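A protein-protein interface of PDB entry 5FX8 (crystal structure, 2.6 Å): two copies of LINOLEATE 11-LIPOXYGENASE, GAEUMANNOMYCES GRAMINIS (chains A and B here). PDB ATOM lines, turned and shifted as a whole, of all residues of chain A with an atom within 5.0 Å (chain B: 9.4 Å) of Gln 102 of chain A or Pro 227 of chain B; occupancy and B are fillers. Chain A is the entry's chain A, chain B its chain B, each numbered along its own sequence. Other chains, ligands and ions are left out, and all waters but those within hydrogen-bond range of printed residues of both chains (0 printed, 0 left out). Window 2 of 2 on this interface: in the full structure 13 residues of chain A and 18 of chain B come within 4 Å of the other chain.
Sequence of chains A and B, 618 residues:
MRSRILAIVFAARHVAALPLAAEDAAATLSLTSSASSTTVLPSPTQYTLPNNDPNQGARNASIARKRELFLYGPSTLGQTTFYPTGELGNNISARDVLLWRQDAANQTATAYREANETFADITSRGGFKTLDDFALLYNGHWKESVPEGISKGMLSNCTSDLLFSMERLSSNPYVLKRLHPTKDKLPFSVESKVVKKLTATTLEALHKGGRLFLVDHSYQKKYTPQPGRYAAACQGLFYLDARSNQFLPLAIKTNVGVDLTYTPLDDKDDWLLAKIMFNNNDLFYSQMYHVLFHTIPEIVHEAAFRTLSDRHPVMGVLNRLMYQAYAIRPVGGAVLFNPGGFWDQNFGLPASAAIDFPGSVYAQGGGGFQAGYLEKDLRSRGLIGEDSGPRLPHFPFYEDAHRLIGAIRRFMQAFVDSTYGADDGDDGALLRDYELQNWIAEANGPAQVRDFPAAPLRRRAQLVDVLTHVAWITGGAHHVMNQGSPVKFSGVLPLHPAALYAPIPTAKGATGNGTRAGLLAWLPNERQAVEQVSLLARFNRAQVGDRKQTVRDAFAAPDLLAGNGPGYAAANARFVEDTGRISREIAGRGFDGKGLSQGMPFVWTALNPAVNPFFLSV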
ATOM      1  N   LEU A  98     -10.999 -23.538 -21.038  1.00  0.00           N
ATOM      2  CA  LEU A  98      -9.756 -23.206 -20.355  1.00  0.00           C
ATOM      3  C   LEU A  98      -8.762 -22.501 -21.281  1.00  0.00           C
ATOM      4  O   LEU A  98      -8.192 -21.454 -20.930  1.00  0.00           O
ATOM      5  CB  LEU A  98      -9.155 -24.484 -19.804  1.00  0.00           C
ATOM      6  CG  LEU A  98      -8.484 -24.358 -18.464  1.00  0.00           C
ATOM      7  CD1 LEU A  98      -9.478 -23.800 -17.435  1.00  0.00           C
ATOM      8  CD2 LEU A  98      -8.013 -25.730 -18.099  1.00  0.00           C
ATOM      9  N   LEU A  99      -8.524 -23.079 -22.459  1.00  0.00           N
ATOM     10  CA  LEU A  99      -7.630 -22.454 -23.425  1.00  0.00           C
ATOM     11  C   LEU A  99      -8.093 -21.049 -23.786  1.00  0.00           C
ATOM     12  O   LEU A  99      -7.293 -20.107 -23.812  1.00  0.00           O
ATOM     13  CB  LEU A  99      -7.532 -23.335 -24.665  1.00  0.00           C
ATOM     14  CG  LEU A  99      -6.837 -24.677 -24.481  1.00  0.00           C
ATOM     15  CD1 LEU A  99      -7.066 -25.605 -25.678  1.00  0.00           C
ATOM     16  CD2 LEU A  99      -5.374 -24.430 -24.239  1.00  0.00           C
ATOM     17  N   TRP A 100      -9.385 -20.886 -24.044  1.00  0.00           N
ATOM     18  CA  TRP A 100      -9.931 -19.577 -24.350  1.00  0.00           C
ATOM     19  C   TRP A 100      -9.715 -18.588 -23.210  1.00  0.00           C
ATOM     20  O   TRP A 100      -9.341 -17.437 -23.452  1.00  0.00           O
ATOM     21  CB  TRP A 100     -11.410 -19.728 -24.675  1.00  0.00           C
ATOM     22  CG  TRP A 100     -11.957 -18.591 -25.384  1.00  0.00           C
ATOM     23  CD1 TRP A 100     -12.095 -18.468 -26.706  1.00  0.00           C
ATOM     24  CD2 TRP A 100     -12.452 -17.384 -24.803  1.00  0.00           C
ATOM     25  NE1 TRP A 100     -12.646 -17.257 -27.010  1.00  0.00           N
ATOM     26  CE2 TRP A 100     -12.881 -16.568 -25.858  1.00  0.00           C
ATOM     27  CE3 TRP A 100     -12.581 -16.915 -23.485  1.00  0.00           C
ATOM     28  CZ2 TRP A 100     -13.423 -15.309 -25.659  1.00  0.00           C
ATOM     29  CZ3 TRP A 100     -13.114 -15.660 -23.286  1.00  0.00           C
ATOM     30  CH2 TRP A 100     -13.528 -14.867 -24.371  1.00  0.00           C
ATOM     31  N   ARG A 101      -9.970 -19.004 -21.966  1.00  0.00           N
ATOM     32  CA  ARG A 101      -9.694 -18.160 -20.801  1.00  0.00           C
ATOM     33  C   ARG A 101      -8.258 -17.658 -20.807  1.00  0.00           C
ATOM     34  O   ARG A 101      -7.999 -16.476 -20.559  1.00  0.00           O
ATOM     35  CB  ARG A 101      -9.925 -18.928 -19.490  1.00  0.00           C
ATOM     36  CG  ARG A 101     -11.329 -19.052 -18.955  1.00  0.00           C
ATOM     37  CD  ARG A 101     -11.320 -19.534 -17.488  1.00  0.00           C
ATOM     38  NE  ARG A 101     -12.656 -19.337 -16.952  1.00  0.00           N
ATOM     39  CZ  ARG A 101     -13.499 -20.322 -16.737  1.00  0.00           C
ATOM     40  NH1 ARG A 101     -13.104 -21.576 -16.951  1.00  0.00           N
ATOM     41  NH2 ARG A 101     -14.719 -20.068 -16.291  1.00  0.00           N
ATOM     42  N   GLN A 102      -7.297 -18.557 -21.016  1.00  0.00           N
ATOM     43  CA  GLN A 102      -5.926 -18.079 -20.956  1.00  0.00           C
ATOM     44  C   GLN A 102      -5.568 -17.219 -22.155  1.00  0.00           C
ATOM     45  O   GLN A 102      -4.729 -16.322 -22.028  1.00  0.00           O
ATOM     46  CB  GLN A 102      -4.964 -19.242 -20.808  1.00  0.00           C
ATOM     47  CG  GLN A 102      -4.811 -20.085 -22.011  1.00  0.00           C
ATOM     48  CD  GLN A 102      -3.832 -21.191 -21.775  1.00  0.00           C
ATOM     49  OE1 GLN A 102      -3.459 -21.462 -20.631  1.00  0.00           O
ATOM     50  NE2 GLN A 102      -3.401 -21.842 -22.844  1.00  0.00           N
ATOM     51  N   ASP A 103      -6.224 -17.423 -23.295  1.00  0.00           N
ATOM     52  CA  ASP A 103      -5.948 -16.645 -24.485  1.00  0.00           C
ATOM     53  C   ASP A 103      -6.662 -15.303 -24.539  1.00  0.00           C
ATOM     54  O   ASP A 103      -6.263 -14.473 -25.351  1.00  0.00           O
ATOM     55  CB  ASP A 103      -6.301 -17.457 -25.728  1.00  0.00           C
ATOM     56  CG  ASP A 103      -5.206 -18.417 -26.110  1.00  0.00           C
ATOM     57  OD1 ASP A 103      -4.247 -18.508 -25.333  1.00  0.00           O
ATOM     58  OD2 ASP A 103      -5.284 -19.089 -27.157  1.00  0.00           O
ATOM     59  N   ALA A 104      -7.693 -15.052 -23.716  1.00  0.00           N
ATOM     60  CA  ALA A 104      -8.423 -13.777 -23.731  1.00  0.00           C
ATOM     61  C   ALA A 104      -7.910 -12.742 -22.740  1.00  0.00           C
ATOM     62  O   ALA A 104      -8.198 -11.556 -22.902  1.00  0.00           O
ATOM     63  CB  ALA A 104      -9.903 -14.000 -23.442  1.00  0.00           C
ATOM     64  N   ALA A 105      -7.158 -13.163 -21.730  1.00  0.00           N
ATOM     65  CA  ALA A 105      -6.750 -12.272 -20.658  1.00  0.00           C
ATOM     66  C   ALA A 105      -6.022 -11.039 -21.183  1.00  0.00           C
ATOM     67  O   ALA A 105      -6.367  -9.905 -20.841  1.00  0.00           O
ATOM     68  CB  ALA A 105      -5.882 -13.051 -19.676  1.00  0.00           C
ATOM     69  N   ARG A 547       1.746 -15.585 -31.291  1.00  0.00           N
ATOM     70  CA  ARG A 547       1.349 -16.916 -30.874  1.00  0.00           C
ATOM     71  C   ARG A 547       1.516 -17.968 -31.971  1.00  0.00           C
ATOM     72  O   ARG A 547       1.343 -19.157 -31.692  1.00  0.00           O
ATOM     73  CB  ARG A 547      -0.094 -16.868 -30.375  1.00  0.00           C
ATOM     74  CG  ARG A 547      -0.252 -16.055 -29.091  1.00  0.00           C
ATOM     75  CD  ARG A 547      -1.674 -15.970 -28.621  1.00  0.00           C
ATOM     76  NE  ARG A 547      -1.780 -15.377 -27.289  1.00  0.00           N
ATOM     77  CZ  ARG A 547      -2.919 -14.995 -26.715  1.00  0.00           C
ATOM     78  NH1 ARG A 547      -4.073 -15.122 -27.346  1.00  0.00           N
ATOM     79  NH2 ARG A 547      -2.904 -14.461 -25.522  1.00  0.00           N
ATOM     80  N   THR B 224      -7.809 -26.993  -9.783  1.00  0.00           N
ATOM     81  CA  THR B 224      -6.652 -27.178 -10.635  1.00  0.00           C
ATOM     82  C   THR B 224      -6.223 -25.833 -11.186  1.00  0.00           C
ATOM     83  O   THR B 224      -7.029 -25.160 -11.830  1.00  0.00           O
ATOM     84  CB  THR B 224      -6.965 -28.152 -11.770  1.00  0.00           C
ATOM     85  OG1 THR B 224      -7.428 -29.382 -11.216  1.00  0.00           O
ATOM     86  CG2 THR B 224      -5.743 -28.430 -12.598  1.00  0.00           C
ATOM     87  N   PRO B 225      -4.988 -25.407 -10.969  1.00  0.00           N
ATOM     88  CA  PRO B 225      -4.579 -24.066 -11.389  1.00  0.00           C
ATOM     89  C   PRO B 225      -4.590 -23.905 -12.895  1.00  0.00           C
ATOM     90  O   PRO B 225      -4.555 -24.879 -13.646  1.00  0.00           O
ATOM     91  CB  PRO B 225      -3.163 -23.952 -10.839  1.00  0.00           C
ATOM     92  CG  PRO B 225      -3.104 -24.929  -9.729  1.00  0.00           C
ATOM     93  CD  PRO B 225      -3.983 -26.053 -10.114  1.00  0.00           C
ATOM     94  N   GLN B 226      -4.662 -22.644 -13.331  1.00  0.00           N
ATOM     95  CA  GLN B 226      -4.553 -22.320 -14.748  1.00  0.00           C
ATOM     96  C   GLN B 226      -3.211 -22.792 -15.276  1.00  0.00           C
ATOM     97  O   GLN B 226      -2.230 -22.857 -14.526  1.00  0.00           O
ATOM     98  CB  GLN B 226      -4.645 -20.822 -15.003  1.00  0.00           C
ATOM     99  CG  GLN B 226      -5.918 -20.223 -14.577  1.00  0.00           C
ATOM    100  CD  GLN B 226      -5.984 -18.748 -14.848  1.00  0.00           C
ATOM    101  OE1 GLN B 226      -6.326 -18.327 -15.957  1.00  0.00           O
ATOM    102  NE2 GLN B 226      -5.714 -17.941 -13.825  1.00  0.00           N
ATOM    103  N   PRO B 227      -3.134 -23.094 -16.564  1.00  0.00           N
ATOM    104  CA  PRO B 227      -1.870 -23.556 -17.134  1.00  0.00           C
ATOM    105  C   PRO B 227      -0.776 -22.533 -16.904  1.00  0.00           C
ATOM    106  O   PRO B 227      -0.975 -21.341 -17.105  1.00  0.00           O
ATOM    107  CB  PRO B 227      -2.206 -23.714 -18.614  1.00  0.00           C
ATOM    108  CG  PRO B 227      -3.640 -24.000 -18.619  1.00  0.00           C
ATOM    109  CD  PRO B 227      -4.236 -23.198 -17.529  1.00  0.00           C
ATOM    110  N   GLY B 228       0.369 -23.004 -16.444  1.00  0.00           N
ATOM    111  CA  GLY B 228       1.469 -22.122 -16.153  1.00  0.00           C
ATOM    112  C   GLY B 228       1.445 -21.521 -14.767  1.00  0.00           C
ATOM    113  O   GLY B 228       2.334 -20.743 -14.432  1.00  0.00           O
ATOM    114  N   ARG B 229       0.458 -21.855 -13.950  1.00  0.00           N
ATOM    115  CA  ARG B 229       0.392 -21.377 -12.585  1.00  0.00           C
ATOM    116  C   ARG B 229       0.160 -22.561 -11.658  1.00  0.00           C
ATOM    117  O   ARG B 229      -0.308 -23.617 -12.079  1.00  0.00           O
ATOM    118  CB  ARG B 229      -0.684 -20.309 -12.451  1.00  0.00           C
ATOM    119  CG  ARG B 229      -0.345 -19.087 -13.287  1.00  0.00           C
ATOM    120  CD  ARG B 229      -1.551 -18.278 -13.517  1.00  0.00           C
ATOM    121  NE  ARG B 229      -1.237 -17.005 -14.130  1.00  0.00           N
ATOM    122  CZ  ARG B 229      -2.049 -15.948 -14.104  1.00  0.00           C
ATOM    123  NH1 ARG B 229      -3.213 -16.022 -13.484  1.00  0.00           N
ATOM    124  NH2 ARG B 229      -1.676 -14.814 -14.690  1.00  0.00           N
ATOM    125  N   TYR B 230       0.554 -22.390 -10.394  1.00  0.00           N
ATOM    126  CA  TYR B 230       0.617 -23.488  -9.436  1.00  0.00           C
ATOM    127  C   TYR B 230       0.055 -23.019  -8.102  1.00  0.00           C
ATOM    128  O   TYR B 230      -0.137 -21.825  -7.884  1.00  0.00           O
ATOM    129  CB  TYR B 230       2.063 -24.006  -9.313  1.00  0.00           C
ATOM    130  CG  TYR B 230       2.667 -24.318 -10.669  1.00  0.00           C
ATOM    131  CD1 TYR B 230       3.288 -23.326 -11.427  1.00  0.00           C
ATOM    132  CD2 TYR B 230       2.577 -25.593 -11.208  1.00  0.00           C
ATOM    133  CE1 TYR B 230       3.800 -23.594 -12.671  1.00  0.00           C
ATOM    134  CE2 TYR B 230       3.097 -25.879 -12.432  1.00  0.00           C
ATOM    135  CZ  TYR B 230       3.706 -24.878 -13.169  1.00  0.00           C
ATOM    136  OH  TYR B 230       4.219 -25.187 -14.404  1.00  0.00           O
ATOM    137  N   ASN B 338     -15.678 -13.148 -15.332  1.00  0.00           N
ATOM    138  CA  ASN B 338     -15.883 -13.606 -16.696  1.00  0.00           C
ATOM    139  C   ASN B 338     -14.631 -14.317 -17.225  1.00  0.00           C
ATOM    140  O   ASN B 338     -13.506 -13.980 -16.844  1.00  0.00           O
ATOM    141  CB  ASN B 338     -16.173 -12.433 -17.589  1.00  0.00           C
ATOM    142  CG  ASN B 338     -15.112 -11.418 -17.472  1.00  0.00           C
ATOM    143  OD1 ASN B 338     -14.730 -11.094 -16.364  1.00  0.00           O
ATOM    144  ND2 ASN B 338     -14.567 -10.963 -18.580  1.00  0.00           N
ATOM    145  N   PRO B 339     -14.794 -15.264 -18.149  1.00  0.00           N
ATOM    146  CA  PRO B 339     -13.626 -15.975 -18.700  1.00  0.00           C
ATOM    147  C   PRO B 339     -12.642 -15.008 -19.344  1.00  0.00           C
ATOM    148  O   PRO B 339     -12.990 -14.232 -20.235  1.00  0.00           O
ATOM    149  CB  PRO B 339     -14.246 -16.918 -19.739  1.00  0.00           C
ATOM    150  CG  PRO B 339     -15.659 -16.991 -19.422  1.00  0.00           C
ATOM    151  CD  PRO B 339     -16.045 -15.698 -18.788  1.00  0.00           C
ATOM    152  N   GLY B 340     -11.404 -15.050 -18.873  1.00  0.00           N
ATOM    153  CA  GLY B 340     -10.408 -14.110 -19.327  1.00  0.00           C
ATOM    154  C   GLY B 340     -10.440 -12.746 -18.672  1.00  0.00           C
ATOM    155  O   GLY B 340      -9.761 -11.841 -19.165  1.00  0.00           O
ATOM    156  N   GLY B 341     -11.201 -12.564 -17.586  1.00  0.00           N
ATOM    157  CA  GLY B 341     -11.233 -11.313 -16.869  1.00  0.00           C
ATOM    158  C   GLY B 341     -10.094 -11.186 -15.869  1.00  0.00           C
ATOM    159  O   GLY B 341      -9.131 -11.958 -15.856  1.00  0.00           O
ATOM    160  N   ASP B 344      -8.961 -14.338 -13.785  1.00  0.00           N
ATOM    161  CA  ASP B 344      -8.146 -15.196 -14.640  1.00  0.00           C
ATOM    162  C   ASP B 344      -6.773 -14.588 -14.900  1.00  0.00           C
ATOM    163  O   ASP B 344      -5.758 -15.276 -14.822  1.00  0.00           O
ATOM    164  CB  ASP B 344      -8.857 -15.457 -15.962  1.00  0.00           C
ATOM    165  CG  ASP B 344     -10.008 -16.426 -15.829  1.00  0.00           C
ATOM    166  OD1 ASP B 344     -10.030 -17.196 -14.855  1.00  0.00           O
ATOM    167  OD2 ASP B 344     -10.879 -16.422 -16.715  1.00  0.00           O
ATOM    168  N   GLN B 345      -6.716 -13.291 -15.164  1.00  0.00           N
ATOM    169  CA  GLN B 345      -5.442 -12.682 -15.497  1.00  0.00           C
ATOM    170  C   GLN B 345      -4.448 -12.686 -14.345  1.00  0.00           C
ATOM    171  O   GLN B 345      -3.257 -12.511 -14.591  1.00  0.00           O
ATOM    172  CB  GLN B 345      -5.665 -11.263 -15.968  1.00  0.00           C
ATOM    173  CG  GLN B 345      -4.547 -10.739 -16.793  1.00  0.00           C
ATOM    174  CD  GLN B 345      -4.549  -9.239 -16.889  1.00  0.00           C
ATOM    175  OE1 GLN B 345      -5.326  -8.553 -16.215  1.00  0.00           O
ATOM    176  NE2 GLN B 345      -3.684  -8.709 -17.750  1.00  0.00           N
ATOM    177  N   PHE B 347      -4.994 -14.604 -10.813  1.00  0.00           N
ATOM    178  CA  PHE B 347      -4.986 -15.622  -9.780  1.00  0.00           C
ATOM    179  C   PHE B 347      -4.650 -17.001 -10.338  1.00  0.00           C
ATOM    180  O   PHE B 347      -4.919 -17.315 -11.500  1.00  0.00           O
ATOM    181  CB  PHE B 347      -6.333 -15.647  -9.057  1.00  0.00           C
ATOM    182  CG  PHE B 347      -6.553 -14.460  -8.168  1.00  0.00           C
ATOM    183  CD1 PHE B 347      -6.995 -13.265  -8.687  1.00  0.00           C
ATOM    184  CD2 PHE B 347      -6.285 -14.529  -6.827  1.00  0.00           C
ATOM    185  CE1 PHE B 347      -7.186 -12.183  -7.870  1.00  0.00           C
ATOM    186  CE2 PHE B 347      -6.467 -13.448  -6.019  1.00  0.00           C
ATOM    187  CZ  PHE B 347      -6.914 -12.285  -6.531  1.00  0.00           C
ATOM    188  N   GLY B 348      -4.054 -17.829  -9.481  1.00  0.00           N
ATOM    189  CA  GLY B 348      -3.556 -19.115  -9.941  1.00  0.00           C
ATOM    190  C   GLY B 348      -4.662 -20.083 -10.304  1.00  0.00           C
ATOM    191  O   GLY B 348      -4.524 -20.867 -11.238  1.00  0.00           O
ATOM    192  N   LEU B 349      -5.676 -20.068  -9.606  1.00  0.00           N
ATOM    193  CA  LEU B 349      -6.871 -20.834  -9.880  1.00  0.00           C
ATOM    194  C   LEU B 349      -7.759 -20.070 -10.847  1.00  0.00           C
ATOM    195  O   LEU B 349      -7.834 -18.850 -10.785  1.00  0.00           O
ATOM    196  CB  LEU B 349      -7.634 -21.116  -8.600  1.00  0.00           C
ATOM    197  CG  LEU B 349      -6.883 -21.938  -7.548  1.00  0.00           C
ATOM    198  CD1 LEU B 349      -7.806 -22.225  -6.418  1.00  0.00           C
ATOM    199  CD2 LEU B 349      -6.325 -23.240  -8.100  1.00  0.00           C
ATOM    200  N   PRO B 350      -8.437 -20.730 -11.762  1.00  0.00           N
ATOM    201  CA  PRO B 350      -9.290 -20.008 -12.699  1.00  0.00           C
ATOM    202  C   PRO B 350     -10.557 -19.514 -12.004  1.00  0.00           C
ATOM    203  O   PRO B 350     -10.873 -19.905 -10.875  1.00  0.00           O
ATOM    204  CB  PRO B 350      -9.574 -21.070 -13.757  1.00  0.00           C
ATOM    205  CG  PRO B 350      -9.596 -22.320 -12.981  1.00  0.00           C
ATOM    206  CD  PRO B 350      -8.561 -22.188 -11.914  1.00  0.00           C
ATOM    207  N   ALA B 351     -11.297 -18.638 -12.703  1.00  0.00           N
ATOM    208  CA  ALA B 351     -12.494 -18.020 -12.126  1.00  0.00           C
ATOM    209  C   ALA B 351     -13.605 -19.029 -11.911  1.00  0.00           C
ATOM    210  O   ALA B 351     -14.507 -18.789 -11.103  1.00  0.00           O
ATOM    211  CB  ALA B 351     -13.018 -16.873 -12.996  1.00  0.00           C
ATOM    212  N   ALA B 499      -0.798 -15.492  -7.681  1.00  0.00           N
ATOM    213  CA  ALA B 499      -0.519 -16.771  -8.321  1.00  0.00           C
ATOM    214  C   ALA B 499       0.917 -17.157  -8.034  1.00  0.00           C
ATOM    215  O   ALA B 499       1.761 -16.302  -7.784  1.00  0.00           O
ATOM    216  CB  ALA B 499      -0.744 -16.734  -9.832  1.00  0.00           C
ATOM    217  N   LEU B 500       1.183 -18.452  -8.049  1.00  0.00           N
ATOM    218  CA  LEU B 500       2.548 -18.955  -8.059  1.00  0.00           C
ATOM    219  C   LEU B 500       2.882 -19.385  -9.472  1.00  0.00           C
ATOM    220  O   LEU B 500       2.037 -19.955 -10.164  1.00  0.00           O
ATOM    221  CB  LEU B 500       2.723 -20.142  -7.114  1.00  0.00           C
ATOM    222  CG  LEU B 500       2.158 -19.985  -5.714  1.00  0.00           C
ATOM    223  CD1 LEU B 500       2.638 -21.144  -4.901  1.00  0.00           C
ATOM    224  CD2 LEU B 500       2.566 -18.670  -5.094  1.00  0.00           C
ATOM    225  N   TYR B 501       4.125 -19.133  -9.884  1.00  0.00           N
ATOM    226  CA  TYR B 501       4.542 -19.306 -11.273  1.00  0.00           C
ATOM    227  C   TYR B 501       5.575 -20.408 -11.467  1.00  0.00           C
ATOM    228  O   TYR B 501       6.189 -20.471 -12.532  1.00  0.00           O
ATOM    229  CB  TYR B 501       5.068 -17.985 -11.832  1.00  0.00           C
ATOM    230  CG  TYR B 501       3.950 -17.009 -12.050  1.00  0.00           C
ATOM    231  CD1 TYR B 501       3.539 -16.163 -11.032  1.00  0.00           C
ATOM    232  CD2 TYR B 501       3.271 -16.969 -13.249  1.00  0.00           C
ATOM    233  CE1 TYR B 501       2.497 -15.285 -11.206  1.00  0.00           C
ATOM    234  CE2 TYR B 501       2.223 -16.094 -13.442  1.00  0.00           C
ATOM    235  CZ  TYR B 501       1.838 -15.254 -12.416  1.00  0.00           C
ATOM    236  OH  TYR B 501       0.797 -14.390 -12.607  1.00  0.00           O
ATOM    237  N   ALA B 502       5.770 -21.269 -10.471  1.00  0.00           N
ATOM    238  CA  ALA B 502       6.682 -22.406 -10.499  1.00  0.00           C
ATOM    239  C   ALA B 502       6.049 -23.579  -9.767  1.00  0.00           C
ATOM    240  O   ALA B 502       5.212 -23.382  -8.881  1.00  0.00           O
ATOM    241  CB  ALA B 502       8.027 -22.080  -9.840  1.00  0.00           C
ATOM    242  N   GLN B 528       3.509  -8.935 -14.276  1.00  0.00           N
ATOM    243  CA  GLN B 528       2.448  -9.620 -13.549  1.00  0.00           C
ATOM    244  C   GLN B 528       2.287  -9.056 -12.150  1.00  0.00           C
ATOM    245  O   GLN B 528       1.168  -8.964 -11.632  1.00  0.00           O
ATOM    246  CB  GLN B 528       2.736 -11.112 -13.502  1.00  0.00           C
ATOM    247  CG  GLN B 528       2.783 -11.764 -14.849  1.00  0.00           C
ATOM    248  CD  GLN B 528       3.483 -13.087 -14.804  1.00  0.00           C
ATOM    249  OE1 GLN B 528       4.303 -13.332 -13.922  1.00  0.00           O
ATOM    250  NE2 GLN B 528       3.166 -13.957 -15.746  1.00  0.00           N
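OD2 of Asp 344 of chain B is in salt-bridge range of NE of Arg 101 of chain A, at 3.4 Å.
The backbone carbonyl oxygen (O) of Gln 345 of chain B is in hydrogen-bond range of the guanidinium group (NH2) of Arg 229 of chain B. The guanidinium group (NH1) of Arg 229 of chain B is in hydrogen-bond range of the backbone carbonyl oxygen (O) of Asp 344 of chain B. The backbone NH of Gly 340 of chain B is in hydrogen-bond range of the side-chain carboxylate of Asp 344 of chain B (2.6 Å). O of Asp 344 of chain B is in hydrogen-bond range of NE2 of Gln 226 of chain B (2.8 Å). N of Ala 351 of chain B lies within hydrogen-bond range of OD1 of Asp 344 of chain B, at 2.9 Å.
Among the printed residues, merely in contact across the chains: Trp 100 of chain A with Pro 339 of chain B (3.4 Å), Arg 101 of chain A with Pro 339 of chain B (3.7 Å), Arg 101 of chain A with Gly 340 of chain B (3.6 Å), Gln 102 of chain A with Pro 227 of chain B (3.2 Å), Ala 105 of chain A with Gly 340 of chain B (3.4 Å) and Ala 105 of chain A with Gln 345 of chain B (3.9 Å).
Of chain B, only Pro 227 comes within 4 Å of Gln 102 of chain A. Of chain A, only Gln 102 (3.2 Å) comes within 4 Å of Pro 227 of chain B. No residue of chain B comes within 4 Å of Asp 103 of chain A. Of the printed residues of chain A, Asp 344 of chain B touches Arg 101. Of the printed residues of chain A, Gln 345 of chain B touches Ala 105 (3.9 Å). Of the printed residues of chain B, Trp 100 of chain A touches Pro 339. Printed residues of chain A within 4 Å of Pro 339 of chain B: Trp 100 and Arg 101. Of the printed residues of chain B, Arg 101 of chain A touches Pro 339 (3.7 Å), Gly 340 (3.6 Å) and Asp 344 (3.2 Å). The nearest residue of chain B that does not touch Gln 102 of chain A is Gln 226 of chain B (5.0 Å). The nearest residue of chain A that does not touch Pro 227 of chain B is Leu 98 of chain A (4.5 Å).
Of the 9 printed residues of chain A, 4 touch a printed residue of chain B. Hydrophobic or aromatic side chains of chain A that line the printed part of chain B: Trp 100 and Ala 105. Hydrophobic or aromatic side chains of chain B within 4 Å of the printed part of chain A: Pro 227 and Pro 339. Among the printed residues, 7 pairs touch across the chains.
No position is printed for both chains. Of the 7 pairs that touch across the chains among the printed residues, none has its exchanged pair printed and touching as well.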
